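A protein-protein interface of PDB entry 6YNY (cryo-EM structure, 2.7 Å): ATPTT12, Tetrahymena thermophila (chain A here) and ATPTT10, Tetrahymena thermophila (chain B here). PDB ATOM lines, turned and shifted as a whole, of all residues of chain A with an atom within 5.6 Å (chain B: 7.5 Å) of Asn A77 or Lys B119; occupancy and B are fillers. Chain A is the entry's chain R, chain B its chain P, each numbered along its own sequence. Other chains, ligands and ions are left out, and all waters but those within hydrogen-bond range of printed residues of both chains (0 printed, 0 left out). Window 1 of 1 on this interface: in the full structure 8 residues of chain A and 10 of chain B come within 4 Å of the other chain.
Among the printed residues, pairs that only touch across the chains: Asn A75 with Phe B5 (3.9 Å), Asn A75 with Trp B112 (3.1 Å), Gly A76 with Trp B112 (3.6 Å), Asn A77 with Pro B115 (3.6 Å), Asn A77 with Glu B116 (3.6 Å), Asn A77 with Lys B119 (3.4 Å) and Leu A82 with Lys B119 (3.9 Å).
ND2 of Asn A75 is in hydrogen-bond range of O of Val B114. The backbone carbonyl oxygen of Lys B111 sits close to the side-chain amide oxygen of Asn A75. O of Val B114 lies within hydrogen-bond range of ND2 of Asn A77, 2.8 Å away. O of Gly A78 sits at hydrogen-bond distance from NZ of Lys B119 (2.6 Å).
Of the 16 printed residues of chain B, 7 touch a printed residue of chain A. Printed residues of chain B that touch a printed residue of chain A: Phe B5, Lys B111, Trp B112, Val B114, Pro B115, Glu B116 and Lys B119. Hydrophobic or aromatic side chains of chain A that line the printed part of chain B: Leu A82. Among the printed residues, 11 pairs touch across the chains.
O of Phe A72 lies within hydrogen-bond range of N of Gly A78. The side-chain carboxylate of Glu B116 is in salt-bridge range of the side-chain amino group of Lys B119 (2.8 Å). ND2 of Asn B3 lies within hydrogen-bond range of OE1 of Glu B116, at 3.2 Å. O of Phe A72 sits at hydrogen-bond distance from N of Asn A77 (3.2 Å).
Of chain A, only Asn A77, Gly A78 and Leu A82 come within 4 Å of Lys B119. Of chain B, only Trp B112 comes within 4 Å of Gly A76. Of the printed residues of chain B, Gly A78 touches Lys B119. Of the printed residues of chain A, Val B114 touches Asn A75 (3.3 Å) and Asn A77 (2.8 Å). The nearest residue of chain B that does not touch Asn A77 is Phe B5 (5.1 Å). The nearest residue of chain A that does not touch Lys B119 is Gly A79 (4.4 Å). The nearest printed residue of chain A that does not touch Pro B115 is Asn A75 (5.5 Å).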
ATOM      1  N   ILE A  71      28.298  13.462  -4.900  1.00  0.00           N
ATOM      2  CA  ILE A  71      28.269  13.911  -6.284  1.00  0.00           C
ATOM      3  C   ILE A  71      28.525  12.763  -7.245  1.00  0.00           C
ATOM      4  O   ILE A  71      27.788  12.575  -8.215  1.00  0.00           O
ATOM      5  CB  ILE A  71      29.293  15.048  -6.479  1.00  0.00           C
ATOM      6  CG1 ILE A  71      28.864  16.279  -5.686  1.00  0.00           C
ATOM      7  CG2 ILE A  71      29.444  15.377  -7.946  1.00  0.00           C
ATOM      8  CD1 ILE A  71      29.900  17.347  -5.618  1.00  0.00           C
ATOM      9  N   PHE A  72      29.569  11.978  -6.991  1.00  0.00           N
ATOM     10  CA  PHE A  72      29.964  10.910  -7.898  1.00  0.00           C
ATOM     11  C   PHE A  72      29.293   9.586  -7.571  1.00  0.00           C
ATOM     12  O   PHE A  72      28.966   8.818  -8.482  1.00  0.00           O
ATOM     13  CB  PHE A  72      31.481  10.742  -7.862  1.00  0.00           C
ATOM     14  CG  PHE A  72      32.229  11.969  -8.271  1.00  0.00           C
ATOM     15  CD1 PHE A  72      32.489  12.224  -9.600  1.00  0.00           C
ATOM     16  CD2 PHE A  72      32.666  12.873  -7.327  1.00  0.00           C
ATOM     17  CE1 PHE A  72      33.172  13.351  -9.976  1.00  0.00           C
ATOM     18  CE2 PHE A  72      33.350  14.000  -7.702  1.00  0.00           C
ATOM     19  CZ  PHE A  72      33.602  14.239  -9.027  1.00  0.00           C
ATOM     20  N   GLY A  73      29.080   9.301  -6.293  1.00  0.00           N
ATOM     21  CA  GLY A  73      28.410   8.080  -5.904  1.00  0.00           C
ATOM     22  C   GLY A  73      29.354   6.931  -5.635  1.00  0.00           C
ATOM     23  O   GLY A  73      30.494   7.130  -5.206  1.00  0.00           O
ATOM     24  N   ASN A  75      30.286   4.328  -7.951  1.00  0.00           N
ATOM     25  CA  ASN A  75      31.123   3.944  -9.078  1.00  0.00           C
ATOM     26  C   ASN A  75      31.286   5.083 -10.076  1.00  0.00           C
ATOM     27  O   ASN A  75      31.356   4.868 -11.287  1.00  0.00           O
ATOM     28  CB  ASN A  75      30.551   2.710  -9.766  1.00  0.00           C
ATOM     29  CG  ASN A  75      31.576   1.980 -10.589  1.00  0.00           C
ATOM     30  OD1 ASN A  75      32.768   2.008 -10.287  1.00  0.00           O
ATOM     31  ND2 ASN A  75      31.121   1.321 -11.639  1.00  0.00           N
ATOM     32  N   GLY A  76      31.346   6.313  -9.580  1.00  0.00           N
ATOM     33  CA  GLY A  76      31.622   7.446 -10.442  1.00  0.00           C
ATOM     34  C   GLY A  76      30.574   7.731 -11.489  1.00  0.00           C
ATOM     35  O   GLY A  76      30.887   8.346 -12.509  1.00  0.00           O
ATOM     36  N   ASN A  77      29.334   7.307 -11.265  1.00  0.00           N
ATOM     37  CA  ASN A  77      28.244   7.550 -12.196  1.00  0.00           C
ATOM     38  C   ASN A  77      27.233   8.561 -11.680  1.00  0.00           C
ATOM     39  O   ASN A  77      26.283   8.886 -12.399  1.00  0.00           O
ATOM     40  CB  ASN A  77      27.530   6.237 -12.524  1.00  0.00           C
ATOM     41  CG  ASN A  77      28.375   5.309 -13.352  1.00  0.00           C
ATOM     42  OD1 ASN A  77      29.131   5.743 -14.218  1.00  0.00           O
ATOM     43  ND2 ASN A  77      28.253   4.018 -13.093  1.00  0.00           N
ATOM     44  N   GLY A  78      27.411   9.069 -10.466  1.00  0.00           N
ATOM     45  CA  GLY A  78      26.477  10.015  -9.898  1.00  0.00           C
ATOM     46  C   GLY A  78      25.845   9.525  -8.615  1.00  0.00           C
ATOM     47  O   GLY A  78      25.452   8.360  -8.506  1.00  0.00           O
ATOM     48  N   GLY A  79      25.743  10.417  -7.636  1.00  0.00           N
ATOM     49  CA  GLY A  79      25.171  10.086  -6.350  1.00  0.00           C
ATOM     50  C   GLY A  79      23.805  10.691  -6.120  1.00  0.00           C
ATOM     51  O   GLY A  79      23.050  10.933  -7.065  1.00  0.00           O
ATOM     52  N   LEU A  82      21.924  13.855  -7.880  1.00  0.00           N
ATOM     53  CA  LEU A  82      21.047  13.783  -9.036  1.00  0.00           C
ATOM     54  C   LEU A  82      19.601  13.478  -8.676  1.00  0.00           C
ATOM     55  O   LEU A  82      18.744  13.488  -9.564  1.00  0.00           O
ATOM     56  CB  LEU A  82      21.553  12.711 -10.002  1.00  0.00           C
ATOM     57  CG  LEU A  82      22.974  12.902 -10.520  1.00  0.00           C
ATOM     58  CD1 LEU A  82      23.426  11.663 -11.246  1.00  0.00           C
ATOM     59  CD2 LEU A  82      23.047  14.106 -11.428  1.00  0.00           C
ATOM     60  N   ASN B   3      19.242  -0.987  -7.009  1.00  0.00           N
ATOM     61  CA  ASN B   3      20.564  -0.453  -7.321  1.00  0.00           C
ATOM     62  C   ASN B   3      21.582  -1.375  -6.660  1.00  0.00           C
ATOM     63  O   ASN B   3      22.009  -1.136  -5.528  1.00  0.00           O
ATOM     64  CB  ASN B   3      20.697   0.987  -6.839  1.00  0.00           C
ATOM     65  CG  ASN B   3      22.027   1.606  -7.209  1.00  0.00           C
ATOM     66  OD1 ASN B   3      23.026   1.420  -6.515  1.00  0.00           O
ATOM     67  ND2 ASN B   3      22.044   2.357  -8.304  1.00  0.00           N
ATOM     68  N   PHE B   5      25.199  -3.739  -7.500  1.00  0.00           N
ATOM     69  CA  PHE B   5      26.293  -4.170  -8.356  1.00  0.00           C
ATOM     70  C   PHE B   5      26.580  -5.642  -8.099  1.00  0.00           C
ATOM     71  O   PHE B   5      26.728  -6.060  -6.947  1.00  0.00           O
ATOM     72  CB  PHE B   5      27.548  -3.339  -8.098  1.00  0.00           C
ATOM     73  CG  PHE B   5      27.431  -1.916  -8.543  1.00  0.00           C
ATOM     74  CD1 PHE B   5      27.789  -1.551  -9.824  1.00  0.00           C
ATOM     75  CD2 PHE B   5      26.971  -0.942  -7.680  1.00  0.00           C
ATOM     76  CE1 PHE B   5      27.685  -0.246 -10.237  1.00  0.00           C
ATOM     77  CE2 PHE B   5      26.866   0.364  -8.090  1.00  0.00           C
ATOM     78  CZ  PHE B   5      27.224   0.713  -9.370  1.00  0.00           C
ATOM     79  N   HIS B  18      25.210  -4.520 -13.396  1.00  0.00           N
ATOM     80  CA  HIS B  18      24.315  -3.768 -12.532  1.00  0.00           C
ATOM     81  C   HIS B  18      22.884  -4.199 -12.807  1.00  0.00           C
ATOM     82  O   HIS B  18      22.512  -4.441 -13.958  1.00  0.00           O
ATOM     83  CB  HIS B  18      24.471  -2.261 -12.761  1.00  0.00           C
ATOM     84  CG  HIS B  18      23.840  -1.415 -11.702  1.00  0.00           C
ATOM     85  ND1 HIS B  18      22.589  -0.858 -11.842  1.00  0.00           N
ATOM     86  CD2 HIS B  18      24.295  -1.016 -10.493  1.00  0.00           C
ATOM     87  CE1 HIS B  18      22.295  -0.163 -10.759  1.00  0.00           C
ATOM     88  NE2 HIS B  18      23.314  -0.241  -9.926  1.00  0.00           N
ATOM     89  N   SER B  20      20.254  -2.603 -12.923  1.00  0.00           N
ATOM     90  CA  SER B  20      19.547  -1.717 -13.836  1.00  0.00           C
ATOM     91  C   SER B  20      19.667  -2.166 -15.283  1.00  0.00           C
ATOM     92  O   SER B  20      18.884  -1.716 -16.126  1.00  0.00           O
ATOM     93  CB  SER B  20      20.074  -0.292 -13.687  1.00  0.00           C
ATOM     94  OG  SER B  20      21.465  -0.234 -13.932  1.00  0.00           O
ATOM     95  N   LYS B 111      34.822  -2.965 -12.682  1.00  0.00           N
ATOM     96  CA  LYS B 111      33.643  -2.382 -12.056  1.00  0.00           C
ATOM     97  C   LYS B 111      33.455  -0.932 -12.476  1.00  0.00           C
ATOM     98  O   LYS B 111      32.322  -0.466 -12.641  1.00  0.00           O
ATOM     99  CB  LYS B 111      33.764  -2.484 -10.539  1.00  0.00           C
ATOM    100  CG  LYS B 111      32.491  -2.176  -9.793  1.00  0.00           C
ATOM    101  CD  LYS B 111      32.751  -2.057  -8.309  1.00  0.00           C
ATOM    102  CE  LYS B 111      31.466  -1.909  -7.532  1.00  0.00           C
ATOM    103  NZ  LYS B 111      30.628  -3.127  -7.657  1.00  0.00           N
ATOM    104  N   TRP B 112      34.556  -0.206 -12.662  1.00  0.00           N
ATOM    105  CA  TRP B 112      34.475   1.206 -13.011  1.00  0.00           C
ATOM    106  C   TRP B 112      33.825   1.431 -14.366  1.00  0.00           C
ATOM    107  O   TRP B 112      33.369   2.545 -14.645  1.00  0.00           O
ATOM    108  CB  TRP B 112      35.873   1.816 -12.987  1.00  0.00           C
ATOM    109  CG  TRP B 112      35.878   3.300 -13.014  1.00  0.00           C
ATOM    110  CD1 TRP B 112      36.193   4.099 -14.069  1.00  0.00           C
ATOM    111  CD2 TRP B 112      35.548   4.173 -11.932  1.00  0.00           C
ATOM    112  NE1 TRP B 112      36.082   5.419 -13.711  1.00  0.00           N
ATOM    113  CE2 TRP B 112      35.686   5.490 -12.403  1.00  0.00           C
ATOM    114  CE3 TRP B 112      35.149   3.968 -10.610  1.00  0.00           C
ATOM    115  CZ2 TRP B 112      35.440   6.597 -11.599  1.00  0.00           C
ATOM    116  CZ3 TRP B 112      34.907   5.067  -9.815  1.00  0.00           C
ATOM    117  CH2 TRP B 112      35.053   6.364 -10.311  1.00  0.00           C
ATOM    118  N   GLU B 113      33.766   0.407 -15.210  1.00  0.00           N
ATOM    119  CA  GLU B 113      33.149   0.520 -16.522  1.00  0.00           C
ATOM    120  C   GLU B 113      31.649   0.275 -16.491  1.00  0.00           C
ATOM    121  O   GLU B 113      30.988   0.446 -17.519  1.00  0.00           O
ATOM    122  CB  GLU B 113      33.790  -0.473 -17.491  1.00  0.00           C
ATOM    123  CG  GLU B 113      35.280  -0.294 -17.677  1.00  0.00           C
ATOM    124  CD  GLU B 113      35.886  -1.364 -18.564  1.00  0.00           C
ATOM    125  OE1 GLU B 113      35.140  -2.258 -19.013  1.00  0.00           O
ATOM    126  OE2 GLU B 113      37.109  -1.312 -18.811  1.00  0.00           O
ATOM    127  N   VAL B 114      31.102  -0.113 -15.345  1.00  0.00           N
ATOM    128  CA  VAL B 114      29.696  -0.484 -15.230  1.00  0.00           C
ATOM    129  C   VAL B 114      28.836   0.767 -15.113  1.00  0.00           C
ATOM    130  O   VAL B 114      29.005   1.545 -14.164  1.00  0.00           O
ATOM    131  CB  VAL B 114      29.473  -1.411 -14.029  1.00  0.00           C
ATOM    132  CG1 VAL B 114      28.030  -1.832 -13.959  1.00  0.00           C
ATOM    133  CG2 VAL B 114      30.380  -2.605 -14.121  1.00  0.00           C
ATOM    134  N   PRO B 115      27.912   1.005 -16.036  1.00  0.00           N
ATOM    135  CA  PRO B 115      27.025   2.161 -15.921  1.00  0.00           C
ATOM    136  C   PRO B 115      25.738   1.835 -15.178  1.00  0.00           C
ATOM    137  O   PRO B 115      25.282   0.692 -15.124  1.00  0.00           O
ATOM    138  CB  PRO B 115      26.731   2.503 -17.386  1.00  0.00           C
ATOM    139  CG  PRO B 115      26.743   1.193 -18.057  1.00  0.00           C
ATOM    140  CD  PRO B 115      27.737   0.327 -17.331  1.00  0.00           C
ATOM    141  N   GLU B 116      25.158   2.880 -14.599  1.00  0.00           N
ATOM    142  CA  GLU B 116      23.848   2.804 -13.968  1.00  0.00           C
ATOM    143  C   GLU B 116      22.844   3.406 -14.940  1.00  0.00           C
ATOM    144  O   GLU B 116      22.893   4.605 -15.230  1.00  0.00           O
ATOM    145  CB  GLU B 116      23.841   3.535 -12.629  1.00  0.00           C
ATOM    146  CG  GLU B 116      24.871   3.023 -11.642  1.00  0.00           C
ATOM    147  CD  GLU B 116      24.882   3.807 -10.347  1.00  0.00           C
ATOM    148  OE1 GLU B 116      23.846   4.419 -10.011  1.00  0.00           O
ATOM    149  OE2 GLU B 116      25.928   3.820  -9.665  1.00  0.00           O
ATOM    150  N   LEU B 117      21.938   2.571 -15.444  1.00  0.00           N
ATOM    151  CA  LEU B 117      21.015   3.012 -16.481  1.00  0.00           C
ATOM    152  C   LEU B 117      20.205   4.219 -16.037  1.00  0.00           C
ATOM    153  O   LEU B 117      19.852   5.068 -16.863  1.00  0.00           O
ATOM    154  CB  LEU B 117      20.088   1.863 -16.859  1.00  0.00           C
ATOM    155  CG  LEU B 117      19.282   2.025 -18.142  1.00  0.00           C
ATOM    156  CD1 LEU B 117      20.190   2.004 -19.343  1.00  0.00           C
ATOM    157  CD2 LEU B 117      18.262   0.933 -18.242  1.00  0.00           C
ATOM    158  N   SER B 118      19.906   4.314 -14.746  1.00  0.00           N
ATOM    159  CA  SER B 118      19.159   5.440 -14.211  1.00  0.00           C
ATOM    160  C   SER B 118      19.992   6.708 -14.098  1.00  0.00           C
ATOM    161  O   SER B 118      19.424   7.781 -13.870  1.00  0.00           O
ATOM    162  CB  SER B 118      18.599   5.078 -12.838  1.00  0.00           C
ATOM    163  OG  SER B 118      17.873   6.159 -12.288  1.00  0.00           O
ATOM    164  N   LYS B 119      21.309   6.615 -14.257  1.00  0.00           N
ATOM    165  CA  LYS B 119      22.201   7.757 -14.127  1.00  0.00           C
ATOM    166  C   LYS B 119      22.716   8.261 -15.466  1.00  0.00           C
ATOM    167  O   LYS B 119      23.499   9.215 -15.493  1.00  0.00           O
ATOM    168  CB  LYS B 119      23.391   7.395 -13.236  1.00  0.00           C
ATOM    169  CG  LYS B 119      23.024   6.867 -11.873  1.00  0.00           C
ATOM    170  CD  LYS B 119      22.369   7.920 -11.028  1.00  0.00           C
ATOM    171  CE  LYS B 119      22.085   7.398  -9.638  1.00  0.00           C
ATOM    172  NZ  LYS B 119      23.326   6.985  -8.938  1.00  0.00           N
ATOM    173  N   LEU B 120      22.314   7.644 -16.571  1.00  0.00           N
ATOM    174  CA  LEU B 120      22.811   8.036 -17.879  1.00  0.00           C
ATOM    175  C   LEU B 120      22.026   9.219 -18.425  1.00  0.00           C
ATOM    176  O   LEU B 120      20.849   9.414 -18.109  1.00  0.00           O
ATOM    177  CB  LEU B 120      22.725   6.871 -18.861  1.00  0.00           C
ATOM    178  CG  LEU B 120      23.595   5.652 -18.564  1.00  0.00           C
ATOM    179  CD1 LEU B 120      23.363   4.586 -19.597  1.00  0.00           C
ATOM    180  CD2 LEU B 120      25.053   6.023 -18.526  1.00  0.00           C
ATOM    181  N   TYR B 121      22.694  10.010 -19.255  1.00  0.00           N
ATOM    182  CA  TYR B 121      22.075  11.153 -19.902  1.00  0.00           C
ATOM    183  C   TYR B 121      21.381  10.705 -21.177  1.00  0.00           C
ATOM    184  O   TYR B 121      21.918   9.902 -21.944  1.00  0.00           O
ATOM    185  CB  TYR B 121      23.119  12.221 -20.222  1.00  0.00           C
ATOM    186  CG  TYR B 121      22.552  13.508 -20.762  1.00  0.00           C
ATOM    187  CD1 TYR B 121      22.231  14.557 -19.915  1.00  0.00           C
ATOM    188  CD2 TYR B 121      22.346  13.681 -22.118  1.00  0.00           C
ATOM    189  CE1 TYR B 121      21.718  15.734 -20.405  1.00  0.00           C
ATOM    190  CE2 TYR B 121      21.833  14.854 -22.616  1.00  0.00           C
ATOM    191  CZ  TYR B 121      21.521  15.878 -21.756  1.00  0.00           C
ATOM    192  OH  TYR B 121      21.010  17.052 -22.249  1.00  0.00           O
ATOM    193  N   PHE B 122      20.180  11.228 -21.395  1.00  0.00           N
ATOM    194  CA  PHE B 122      19.408  10.895 -22.577  1.00  0.00           C
ATOM    195  C   PHE B 122      18.560  12.093 -22.962  1.00  0.00           C
ATOM    196  O   PHE B 122      18.411  13.050 -22.199  1.00  0.00           O
ATOM    197  CB  PHE B 122      18.533   9.663 -22.352  1.00  0.00           C
ATOM    198  CG  PHE B 122      17.420   9.876 -21.372  1.00  0.00           C
ATOM    199  CD1 PHE B 122      16.168  10.260 -21.802  1.00  0.00           C
ATOM    200  CD2 PHE B 122      17.622   9.681 -20.022  1.00  0.00           C
ATOM    201  CE1 PHE B 122      15.149  10.450 -20.908  1.00  0.00           C
ATOM    202  CE2 PHE B 122      16.604   9.871 -19.128  1.00  0.00           C
ATOM    203  CZ  PHE B 122      15.366  10.255 -19.570  1.00  0.00           C
